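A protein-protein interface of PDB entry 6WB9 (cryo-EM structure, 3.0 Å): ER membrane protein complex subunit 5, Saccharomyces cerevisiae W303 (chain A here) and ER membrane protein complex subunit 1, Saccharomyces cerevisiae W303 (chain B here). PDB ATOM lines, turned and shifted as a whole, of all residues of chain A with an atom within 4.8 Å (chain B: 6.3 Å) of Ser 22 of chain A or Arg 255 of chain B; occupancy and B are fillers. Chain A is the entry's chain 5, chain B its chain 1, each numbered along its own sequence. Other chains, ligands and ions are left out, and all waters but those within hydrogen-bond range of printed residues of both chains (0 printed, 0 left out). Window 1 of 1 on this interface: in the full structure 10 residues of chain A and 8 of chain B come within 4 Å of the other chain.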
ATOM      1  N   HIS A  18      -1.993  24.596 -27.680  1.00  0.00           N
ATOM      2  CA  HIS A  18      -1.405  23.281 -27.449  1.00  0.00           C
ATOM      3  C   HIS A  18      -1.757  22.749 -26.067  1.00  0.00           C
ATOM      4  O   HIS A  18      -2.046  21.558 -25.913  1.00  0.00           O
ATOM      5  CB  HIS A  18       0.110  23.346 -27.626  1.00  0.00           C
ATOM      6  CG  HIS A  18       0.811  22.066 -27.293  1.00  0.00           C
ATOM      7  ND1 HIS A  18       1.816  21.990 -26.355  1.00  0.00           N
ATOM      8  CD2 HIS A  18       0.645  20.810 -27.771  1.00  0.00           C
ATOM      9  CE1 HIS A  18       2.243  20.742 -26.272  1.00  0.00           C
ATOM     10  NE2 HIS A  18       1.549  20.008 -27.120  1.00  0.00           N
ATOM     11  N   SER A  19      -1.793  23.623 -25.060  1.00  0.00           N
ATOM     12  CA  SER A  19      -2.135  23.178 -23.717  1.00  0.00           C
ATOM     13  C   SER A  19      -3.622  22.889 -23.579  1.00  0.00           C
ATOM     14  O   SER A  19      -4.002  21.973 -22.846  1.00  0.00           O
ATOM     15  CB  SER A  19      -1.697  24.220 -22.696  1.00  0.00           C
ATOM     16  OG  SER A  19      -2.067  23.815 -21.394  1.00  0.00           O
ATOM     17  N   GLY A  20      -4.472  23.627 -24.294  1.00  0.00           N
ATOM     18  CA  GLY A  20      -5.888  23.311 -24.297  1.00  0.00           C
ATOM     19  C   GLY A  20      -6.190  22.026 -25.035  1.00  0.00           C
ATOM     20  O   GLY A  20      -7.053  21.255 -24.618  1.00  0.00           O
ATOM     21  N   PHE A  21      -5.461  21.757 -26.122  1.00  0.00           N
ATOM     22  CA  PHE A  21      -5.622  20.487 -26.822  1.00  0.00           C
ATOM     23  C   PHE A  21      -5.112  19.322 -25.982  1.00  0.00           C
ATOM     24  O   PHE A  21      -5.720  18.247 -25.970  1.00  0.00           O
ATOM     25  CB  PHE A  21      -4.899  20.538 -28.164  1.00  0.00           C
ATOM     26  CG  PHE A  21      -4.941  19.247 -28.923  1.00  0.00           C
ATOM     27  CD1 PHE A  21      -6.119  18.814 -29.506  1.00  0.00           C
ATOM     28  CD2 PHE A  21      -3.801  18.473 -29.063  1.00  0.00           C
ATOM     29  CE1 PHE A  21      -6.162  17.627 -30.208  1.00  0.00           C
ATOM     30  CE2 PHE A  21      -3.837  17.287 -29.764  1.00  0.00           C
ATOM     31  CZ  PHE A  21      -5.019  16.863 -30.337  1.00  0.00           C
ATOM     32  N   SER A  22      -4.018  19.531 -25.245  1.00  0.00           N
ATOM     33  CA  SER A  22      -3.499  18.483 -24.374  1.00  0.00           C
ATOM     34  C   SER A  22      -4.430  18.227 -23.192  1.00  0.00           C
ATOM     35  O   SER A  22      -4.631  17.074 -22.793  1.00  0.00           O
ATOM     36  CB  SER A  22      -2.102  18.860 -23.894  1.00  0.00           C
ATOM     37  OG  SER A  22      -1.390  17.719 -23.455  1.00  0.00           O
ATOM     38  N   SER A  23      -5.024  19.285 -22.635  1.00  0.00           N
ATOM     39  CA  SER A  23      -5.989  19.111 -21.556  1.00  0.00           C
ATOM     40  C   SER A  23      -7.287  18.494 -22.056  1.00  0.00           C
ATOM     41  O   SER A  23      -7.932  17.743 -21.319  1.00  0.00           O
ATOM     42  CB  SER A  23      -6.264  20.452 -20.880  1.00  0.00           C
ATOM     43  OG  SER A  23      -7.185  20.304 -19.816  1.00  0.00           O
ATOM     44  N   TYR A  24      -7.673  18.782 -23.303  1.00  0.00           N
ATOM     45  CA  TYR A  24      -8.818  18.118 -23.914  1.00  0.00           C
ATOM     46  C   TYR A  24      -8.562  16.630 -24.090  1.00  0.00           C
ATOM     47  O   TYR A  24      -9.438  15.809 -23.794  1.00  0.00           O
ATOM     48  CB  TYR A  24      -9.138  18.760 -25.263  1.00  0.00           C
ATOM     49  CG  TYR A  24      -9.989  17.901 -26.168  1.00  0.00           C
ATOM     50  CD1 TYR A  24     -11.330  17.684 -25.889  1.00  0.00           C
ATOM     51  CD2 TYR A  24      -9.453  17.314 -27.309  1.00  0.00           C
ATOM     52  CE1 TYR A  24     -12.112  16.900 -26.710  1.00  0.00           C
ATOM     53  CE2 TYR A  24     -10.228  16.527 -28.138  1.00  0.00           C
ATOM     54  CZ  TYR A  24     -11.558  16.326 -27.833  1.00  0.00           C
ATOM     55  OH  TYR A  24     -12.339  15.545 -28.655  1.00  0.00           O
ATOM     56  N   GLU A  25      -7.365  16.274 -24.568  1.00  0.00           N
ATOM     57  CA  GLU A  25      -6.995  14.870 -24.713  1.00  0.00           C
ATOM     58  C   GLU A  25      -6.963  14.159 -23.369  1.00  0.00           C
ATOM     59  O   GLU A  25      -7.452  13.031 -23.249  1.00  0.00           O
ATOM     60  CB  GLU A  25      -5.640  14.755 -25.398  1.00  0.00           C
ATOM     61  CG  GLU A  25      -5.673  15.013 -26.879  1.00  0.00           C
ATOM     62  CD  GLU A  25      -4.370  14.650 -27.541  1.00  0.00           C
ATOM     63  OE1 GLU A  25      -3.332  15.248 -27.187  1.00  0.00           O
ATOM     64  OE2 GLU A  25      -4.381  13.746 -28.400  1.00  0.00           O
ATOM     65  N   PHE A  26      -6.430  14.819 -22.339  1.00  0.00           N
ATOM     66  CA  PHE A  26      -6.363  14.195 -21.022  1.00  0.00           C
ATOM     67  C   PHE A  26      -7.745  14.031 -20.403  1.00  0.00           C
ATOM     68  O   PHE A  26      -8.046  12.982 -19.824  1.00  0.00           O
ATOM     69  CB  PHE A  26      -5.463  15.006 -20.096  1.00  0.00           C
ATOM     70  CG  PHE A  26      -5.294  14.389 -18.745  1.00  0.00           C
ATOM     71  CD1 PHE A  26      -4.436  13.318 -18.569  1.00  0.00           C
ATOM     72  CD2 PHE A  26      -5.999  14.869 -17.652  1.00  0.00           C
ATOM     73  CE1 PHE A  26      -4.282  12.738 -17.333  1.00  0.00           C
ATOM     74  CE2 PHE A  26      -5.852  14.290 -16.416  1.00  0.00           C
ATOM     75  CZ  PHE A  26      -4.991  13.223 -16.258  1.00  0.00           C
ATOM     76  N   ASP A  48       2.851  19.234 -16.147  1.00  0.00           N
ATOM     77  CA  ASP A  48       3.409  19.897 -17.319  1.00  0.00           C
ATOM     78  C   ASP A  48       2.331  20.623 -18.114  1.00  0.00           C
ATOM     79  O   ASP A  48       2.578  21.721 -18.620  1.00  0.00           O
ATOM     80  CB  ASP A  48       4.154  18.893 -18.200  1.00  0.00           C
ATOM     81  CG  ASP A  48       3.287  17.730 -18.617  1.00  0.00           C
ATOM     82  OD1 ASP A  48       2.337  17.406 -17.877  1.00  0.00           O
ATOM     83  OD2 ASP A  48       3.553  17.138 -19.682  1.00  0.00           O
ATOM     84  N   ILE A  49       1.121  20.063 -18.188  1.00  0.00           N
ATOM     85  CA  ILE A  49       0.013  20.747 -18.854  1.00  0.00           C
ATOM     86  C   ILE A  49      -0.446  21.946 -18.031  1.00  0.00           C
ATOM     87  O   ILE A  49      -0.783  23.004 -18.579  1.00  0.00           O
ATOM     88  CB  ILE A  49      -1.138  19.758 -19.114  1.00  0.00           C
ATOM     89  CG1 ILE A  49      -0.637  18.551 -19.903  1.00  0.00           C
ATOM     90  CG2 ILE A  49      -2.279  20.422 -19.866  1.00  0.00           C
ATOM     91  CD1 ILE A  49      -1.697  17.502 -20.141  1.00  0.00           C
ATOM     92  N   GLU A  52       2.126  24.563 -18.518  1.00  0.00           N
ATOM     93  CA  GLU A  52       2.025  25.129 -19.857  1.00  0.00           C
ATOM     94  C   GLU A  52       0.837  26.078 -19.990  1.00  0.00           C
ATOM     95  O   GLU A  52       0.944  27.089 -20.690  1.00  0.00           O
ATOM     96  CB  GLU A  52       1.930  24.014 -20.895  1.00  0.00           C
ATOM     97  CG  GLU A  52       2.241  24.464 -22.305  1.00  0.00           C
ATOM     98  CD  GLU A  52       1.895  23.416 -23.337  1.00  0.00           C
ATOM     99  OE1 GLU A  52       1.116  22.501 -23.008  1.00  0.00           O
ATOM    100  OE2 GLU A  52       2.403  23.504 -24.473  1.00  0.00           O
ATOM    101  N   ASN B 250      10.837  16.520 -19.341  1.00  0.00           N
ATOM    102  CA  ASN B 250      10.854  15.392 -20.266  1.00  0.00           C
ATOM    103  C   ASN B 250       9.446  15.027 -20.715  1.00  0.00           C
ATOM    104  O   ASN B 250       9.228  14.716 -21.891  1.00  0.00           O
ATOM    105  CB  ASN B 250      11.542  14.191 -19.618  1.00  0.00           C
ATOM    106  CG  ASN B 250      12.982  14.478 -19.244  1.00  0.00           C
ATOM    107  OD1 ASN B 250      13.661  15.266 -19.903  1.00  0.00           O
ATOM    108  ND2 ASN B 250      13.455  13.842 -18.180  1.00  0.00           N
ATOM    109  N   ALA B 251       8.472  15.097 -19.800  1.00  0.00           N
ATOM    110  CA  ALA B 251       7.081  14.851 -20.166  1.00  0.00           C
ATOM    111  C   ALA B 251       6.547  15.948 -21.079  1.00  0.00           C
ATOM    112  O   ALA B 251       5.806  15.664 -22.028  1.00  0.00           O
ATOM    113  CB  ALA B 251       6.220  14.735 -18.910  1.00  0.00           C
ATOM    114  N   TYR B 252       6.936  17.202 -20.822  1.00  0.00           N
ATOM    115  CA  TYR B 252       6.507  18.305 -21.677  1.00  0.00           C
ATOM    116  C   TYR B 252       7.113  18.204 -23.072  1.00  0.00           C
ATOM    117  O   TYR B 252       6.427  18.455 -24.069  1.00  0.00           O
ATOM    118  CB  TYR B 252       6.870  19.644 -21.036  1.00  0.00           C
ATOM    119  CG  TYR B 252       6.643  20.824 -21.953  1.00  0.00           C
ATOM    120  CD1 TYR B 252       5.356  21.222 -22.290  1.00  0.00           C
ATOM    121  CD2 TYR B 252       7.712  21.533 -22.487  1.00  0.00           C
ATOM    122  CE1 TYR B 252       5.141  22.294 -23.133  1.00  0.00           C
ATOM    123  CE2 TYR B 252       7.506  22.607 -23.332  1.00  0.00           C
ATOM    124  CZ  TYR B 252       6.217  22.982 -23.650  1.00  0.00           C
ATOM    125  OH  TYR B 252       6.003  24.051 -24.489  1.00  0.00           O
ATOM    126  N   TRP B 253       8.389  17.820 -23.167  1.00  0.00           N
ATOM    127  CA  TRP B 253       9.015  17.681 -24.476  1.00  0.00           C
ATOM    128  C   TRP B 253       8.498  16.457 -25.220  1.00  0.00           C
ATOM    129  O   TRP B 253       8.389  16.491 -26.451  1.00  0.00           O
ATOM    130  CB  TRP B 253      10.535  17.620 -24.339  1.00  0.00           C
ATOM    131  CG  TRP B 253      11.244  17.621 -25.660  1.00  0.00           C
ATOM    132  CD1 TRP B 253      11.938  16.588 -26.219  1.00  0.00           C
ATOM    133  CD2 TRP B 253      11.314  18.703 -26.598  1.00  0.00           C
ATOM    134  NE1 TRP B 253      12.444  16.962 -27.440  1.00  0.00           N
ATOM    135  CE2 TRP B 253      12.074  18.255 -27.696  1.00  0.00           C
ATOM    136  CE3 TRP B 253      10.811  20.008 -26.612  1.00  0.00           C
ATOM    137  CZ2 TRP B 253      12.342  19.064 -28.798  1.00  0.00           C
ATOM    138  CZ3 TRP B 253      11.077  20.809 -27.707  1.00  0.00           C
ATOM    139  CH2 TRP B 253      11.835  20.335 -28.785  1.00  0.00           C
ATOM    140  N   LEU B 254       8.148  15.388 -24.495  1.00  0.00           N
ATOM    141  CA  LEU B 254       7.507  14.235 -25.121  1.00  0.00           C
ATOM    142  C   LEU B 254       6.136  14.605 -25.674  1.00  0.00           C
ATOM    143  O   LEU B 254       5.793  14.222 -26.800  1.00  0.00           O
ATOM    144  CB  LEU B 254       7.401  13.092 -24.108  1.00  0.00           C
ATOM    145  CG  LEU B 254       6.710  11.763 -24.445  1.00  0.00           C
ATOM    146  CD1 LEU B 254       7.423  11.022 -25.572  1.00  0.00           C
ATOM    147  CD2 LEU B 254       6.561  10.869 -23.219  1.00  0.00           C
ATOM    148  N   ARG B 255       5.355  15.375 -24.904  1.00  0.00           N
ATOM    149  CA  ARG B 255       4.053  15.848 -25.368  1.00  0.00           C
ATOM    150  C   ARG B 255       4.184  16.756 -26.583  1.00  0.00           C
ATOM    151  O   ARG B 255       3.433  16.615 -27.557  1.00  0.00           O
ATOM    152  CB  ARG B 255       3.341  16.592 -24.243  1.00  0.00           C
ATOM    153  CG  ARG B 255       2.316  15.785 -23.478  1.00  0.00           C
ATOM    154  CD  ARG B 255       1.624  16.641 -22.426  1.00  0.00           C
ATOM    155  NE  ARG B 255       1.085  17.878 -22.987  1.00  0.00           N
ATOM    156  CZ  ARG B 255       1.526  19.095 -22.687  1.00  0.00           C
ATOM    157  NH1 ARG B 255       2.519  19.250 -21.823  1.00  0.00           N
ATOM    158  NH2 ARG B 255       0.976  20.158 -23.253  1.00  0.00           N
ATOM    159  N   LEU B 256       5.155  17.675 -26.550  1.00  0.00           N
ATOM    160  CA  LEU B 256       5.334  18.619 -27.646  1.00  0.00           C
ATOM    161  C   LEU B 256       5.822  17.923 -28.909  1.00  0.00           C
ATOM    162  O   LEU B 256       5.349  18.229 -30.006  1.00  0.00           O
ATOM    163  CB  LEU B 256       6.303  19.723 -27.228  1.00  0.00           C
ATOM    164  CG  LEU B 256       6.522  20.863 -28.223  1.00  0.00           C
ATOM    165  CD1 LEU B 256       5.201  21.516 -28.588  1.00  0.00           C
ATOM    166  CD2 LEU B 256       7.486  21.885 -27.652  1.00  0.00           C
ATOM    167  N   THR B 257       6.728  16.948 -28.772  1.00  0.00           N
ATOM    168  CA  THR B 257       7.218  16.227 -29.943  1.00  0.00           C
ATOM    169  C   THR B 257       6.154  15.300 -30.518  1.00  0.00           C
ATOM    170  O   THR B 257       6.053  15.162 -31.742  1.00  0.00           O
ATOM    171  CB  THR B 257       8.478  15.439 -29.592  1.00  0.00           C
ATOM    172  OG1 THR B 257       8.317  14.821 -28.310  1.00  0.00           O
ATOM    173  CG2 THR B 257       9.689  16.356 -29.568  1.00  0.00           C
ATOM    174  N   THR B 258       5.338  14.670 -29.663  1.00  0.00           N
ATOM    175  CA  THR B 258       4.283  13.800 -30.177  1.00  0.00           C
ATOM    176  C   THR B 258       3.184  14.602 -30.864  1.00  0.00           C
ATOM    177  O   THR B 258       2.688  14.197 -31.923  1.00  0.00           O
ATOM    178  CB  THR B 258       3.702  12.941 -29.056  1.00  0.00           C
ATOM    179  OG1 THR B 258       3.519  13.739 -27.882  1.00  0.00           O
ATOM    180  CG2 THR B 258       4.627  11.774 -28.739  1.00  0.00           C
ATOM    181  N   ASN B 259       2.819  15.763 -30.308  1.00  0.00           N
ATOM    182  CA  ASN B 259       1.838  16.611 -30.979  1.00  0.00           C
ATOM    183  C   ASN B 259       2.412  17.253 -32.237  1.00  0.00           C
ATOM    184  O   ASN B 259       1.675  17.468 -33.207  1.00  0.00           O
ATOM    185  CB  ASN B 259       1.316  17.675 -30.018  1.00  0.00           C
ATOM    186  CG  ASN B 259       0.473  17.087 -28.908  1.00  0.00           C
ATOM    187  OD1 ASN B 259      -0.692  16.755 -29.110  1.00  0.00           O
ATOM    188  ND2 ASN B 259       1.059  16.956 -27.726  1.00  0.00           N
ATOM    189  N   TRP B 260       3.722  17.520 -32.259  1.00  0.00           N
ATOM    190  CA  TRP B 260       4.372  18.043 -33.455  1.00  0.00           C
ATOM    191  C   TRP B 260       4.371  17.009 -34.572  1.00  0.00           C
ATOM    192  O   TRP B 260       4.058  17.328 -35.725  1.00  0.00           O
ATOM    193  CB  TRP B 260       5.801  18.469 -33.111  1.00  0.00           C
ATOM    194  CG  TRP B 260       6.447  19.389 -34.104  1.00  0.00           C
ATOM    195  CD1 TRP B 260       6.868  19.075 -35.362  1.00  0.00           C
ATOM    196  CD2 TRP B 260       6.776  20.769 -33.906  1.00  0.00           C
ATOM    197  NE1 TRP B 260       7.422  20.176 -35.967  1.00  0.00           N
ATOM    198  CE2 TRP B 260       7.380  21.229 -35.093  1.00  0.00           C
ATOM    199  CE3 TRP B 260       6.613  21.662 -32.842  1.00  0.00           C
ATOM    200  CZ2 TRP B 260       7.821  22.542 -35.246  1.00  0.00           C
ATOM    201  CZ3 TRP B 260       7.051  22.966 -32.997  1.00  0.00           C
ATOM    202  CH2 TRP B 260       7.647  23.393 -34.190  1.00  0.00           C
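NE of Arg 255 of chain B lies within hydrogen-bond range of OG of Ser 22 of chain A (2.5 Å).
The side-chain carboxylate (OD2) of Asp 48 of chain A is in salt-bridge range of the guanidinium group (NH1) of Arg 255 of chain B.
The guanidinium group of Arg 255 of chain B is in salt-bridge range of the side-chain carboxylate of Glu 52 of chain A (3.7 Å).
A ring nitrogen (NE2) of His 18 of chain A lies within hydrogen-bond range of the side-chain amide nitrogen (ND2) of Asn 259 of chain B, 3.1 Å away.
The backbone carbonyl oxygen (O) of Arg 255 of chain B lies within hydrogen-bond range of the side-chain hydroxyl (OG1) of Thr 258 of chain B (2.9 Å).
The backbone carbonyl oxygen of Arg 255 of chain B sits at hydrogen-bond distance from the side-chain amide nitrogen of Asn 259 of chain B, 2.4 Å away.
The side-chain carboxylate (OE2) of Glu 52 of chain A is in hydrogen-bond range of a ring nitrogen (ND1) of His 18 of chain A, at 2.5 Å.
OG of Ser 19 of chain A is in hydrogen-bond range of O of Ile 49 of chain A (3.2 Å).
Among the printed residues, merely in contact across the chains: His 18 of chain A with Arg 255 of chain B (3.3 Å), His 18 of chain A with Leu 256 of chain B (3.8 Å), Phe 21 of chain A with Asn 259 of chain B (3.3 Å), Glu 25 of chain A with Asn 259 of chain B (3.6 Å), Asp 48 of chain A with Ala 251 of chain B (3.5 Å), Asp 48 of chain A with Tyr 252 of chain B (3.6 Å), Ile 49 of chain A with Arg 255 of chain B (3.6 Å) and Glu 52 of chain A with Tyr 252 of chain B (3.3 Å).
Of chain B, only Arg 255 comes within 4 Å of Ser 22 of chain A.
Of the printed residues of chain A, Tyr 252 of chain B touches Asp 48 and Glu 52.
Trp 253 of chain B touches none of the printed residues of chain A.
Arg 255 of chain B touches five residues of chain A.
Printed residues of chain A within 4 Å of Leu 256 of chain B: His 18.
The nearest residue of chain B that does not touch Ser 22 of chain A is Asn 259 of chain B (5.0 Å).
Of the 11 printed residues of chain B, 5 touch a printed residue of chain A.
Hydrophobic or aromatic side chains of chain B that line the printed part of chain A: Ala 251, Tyr 252 and Leu 256.
Of the 12 printed residues of chain A, 7 touch a printed residue of chain B.
Hydrophobic or aromatic side chains of chain A within 4 Å of the printed part of chain B: His 18, Phe 21 and Ile 49.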
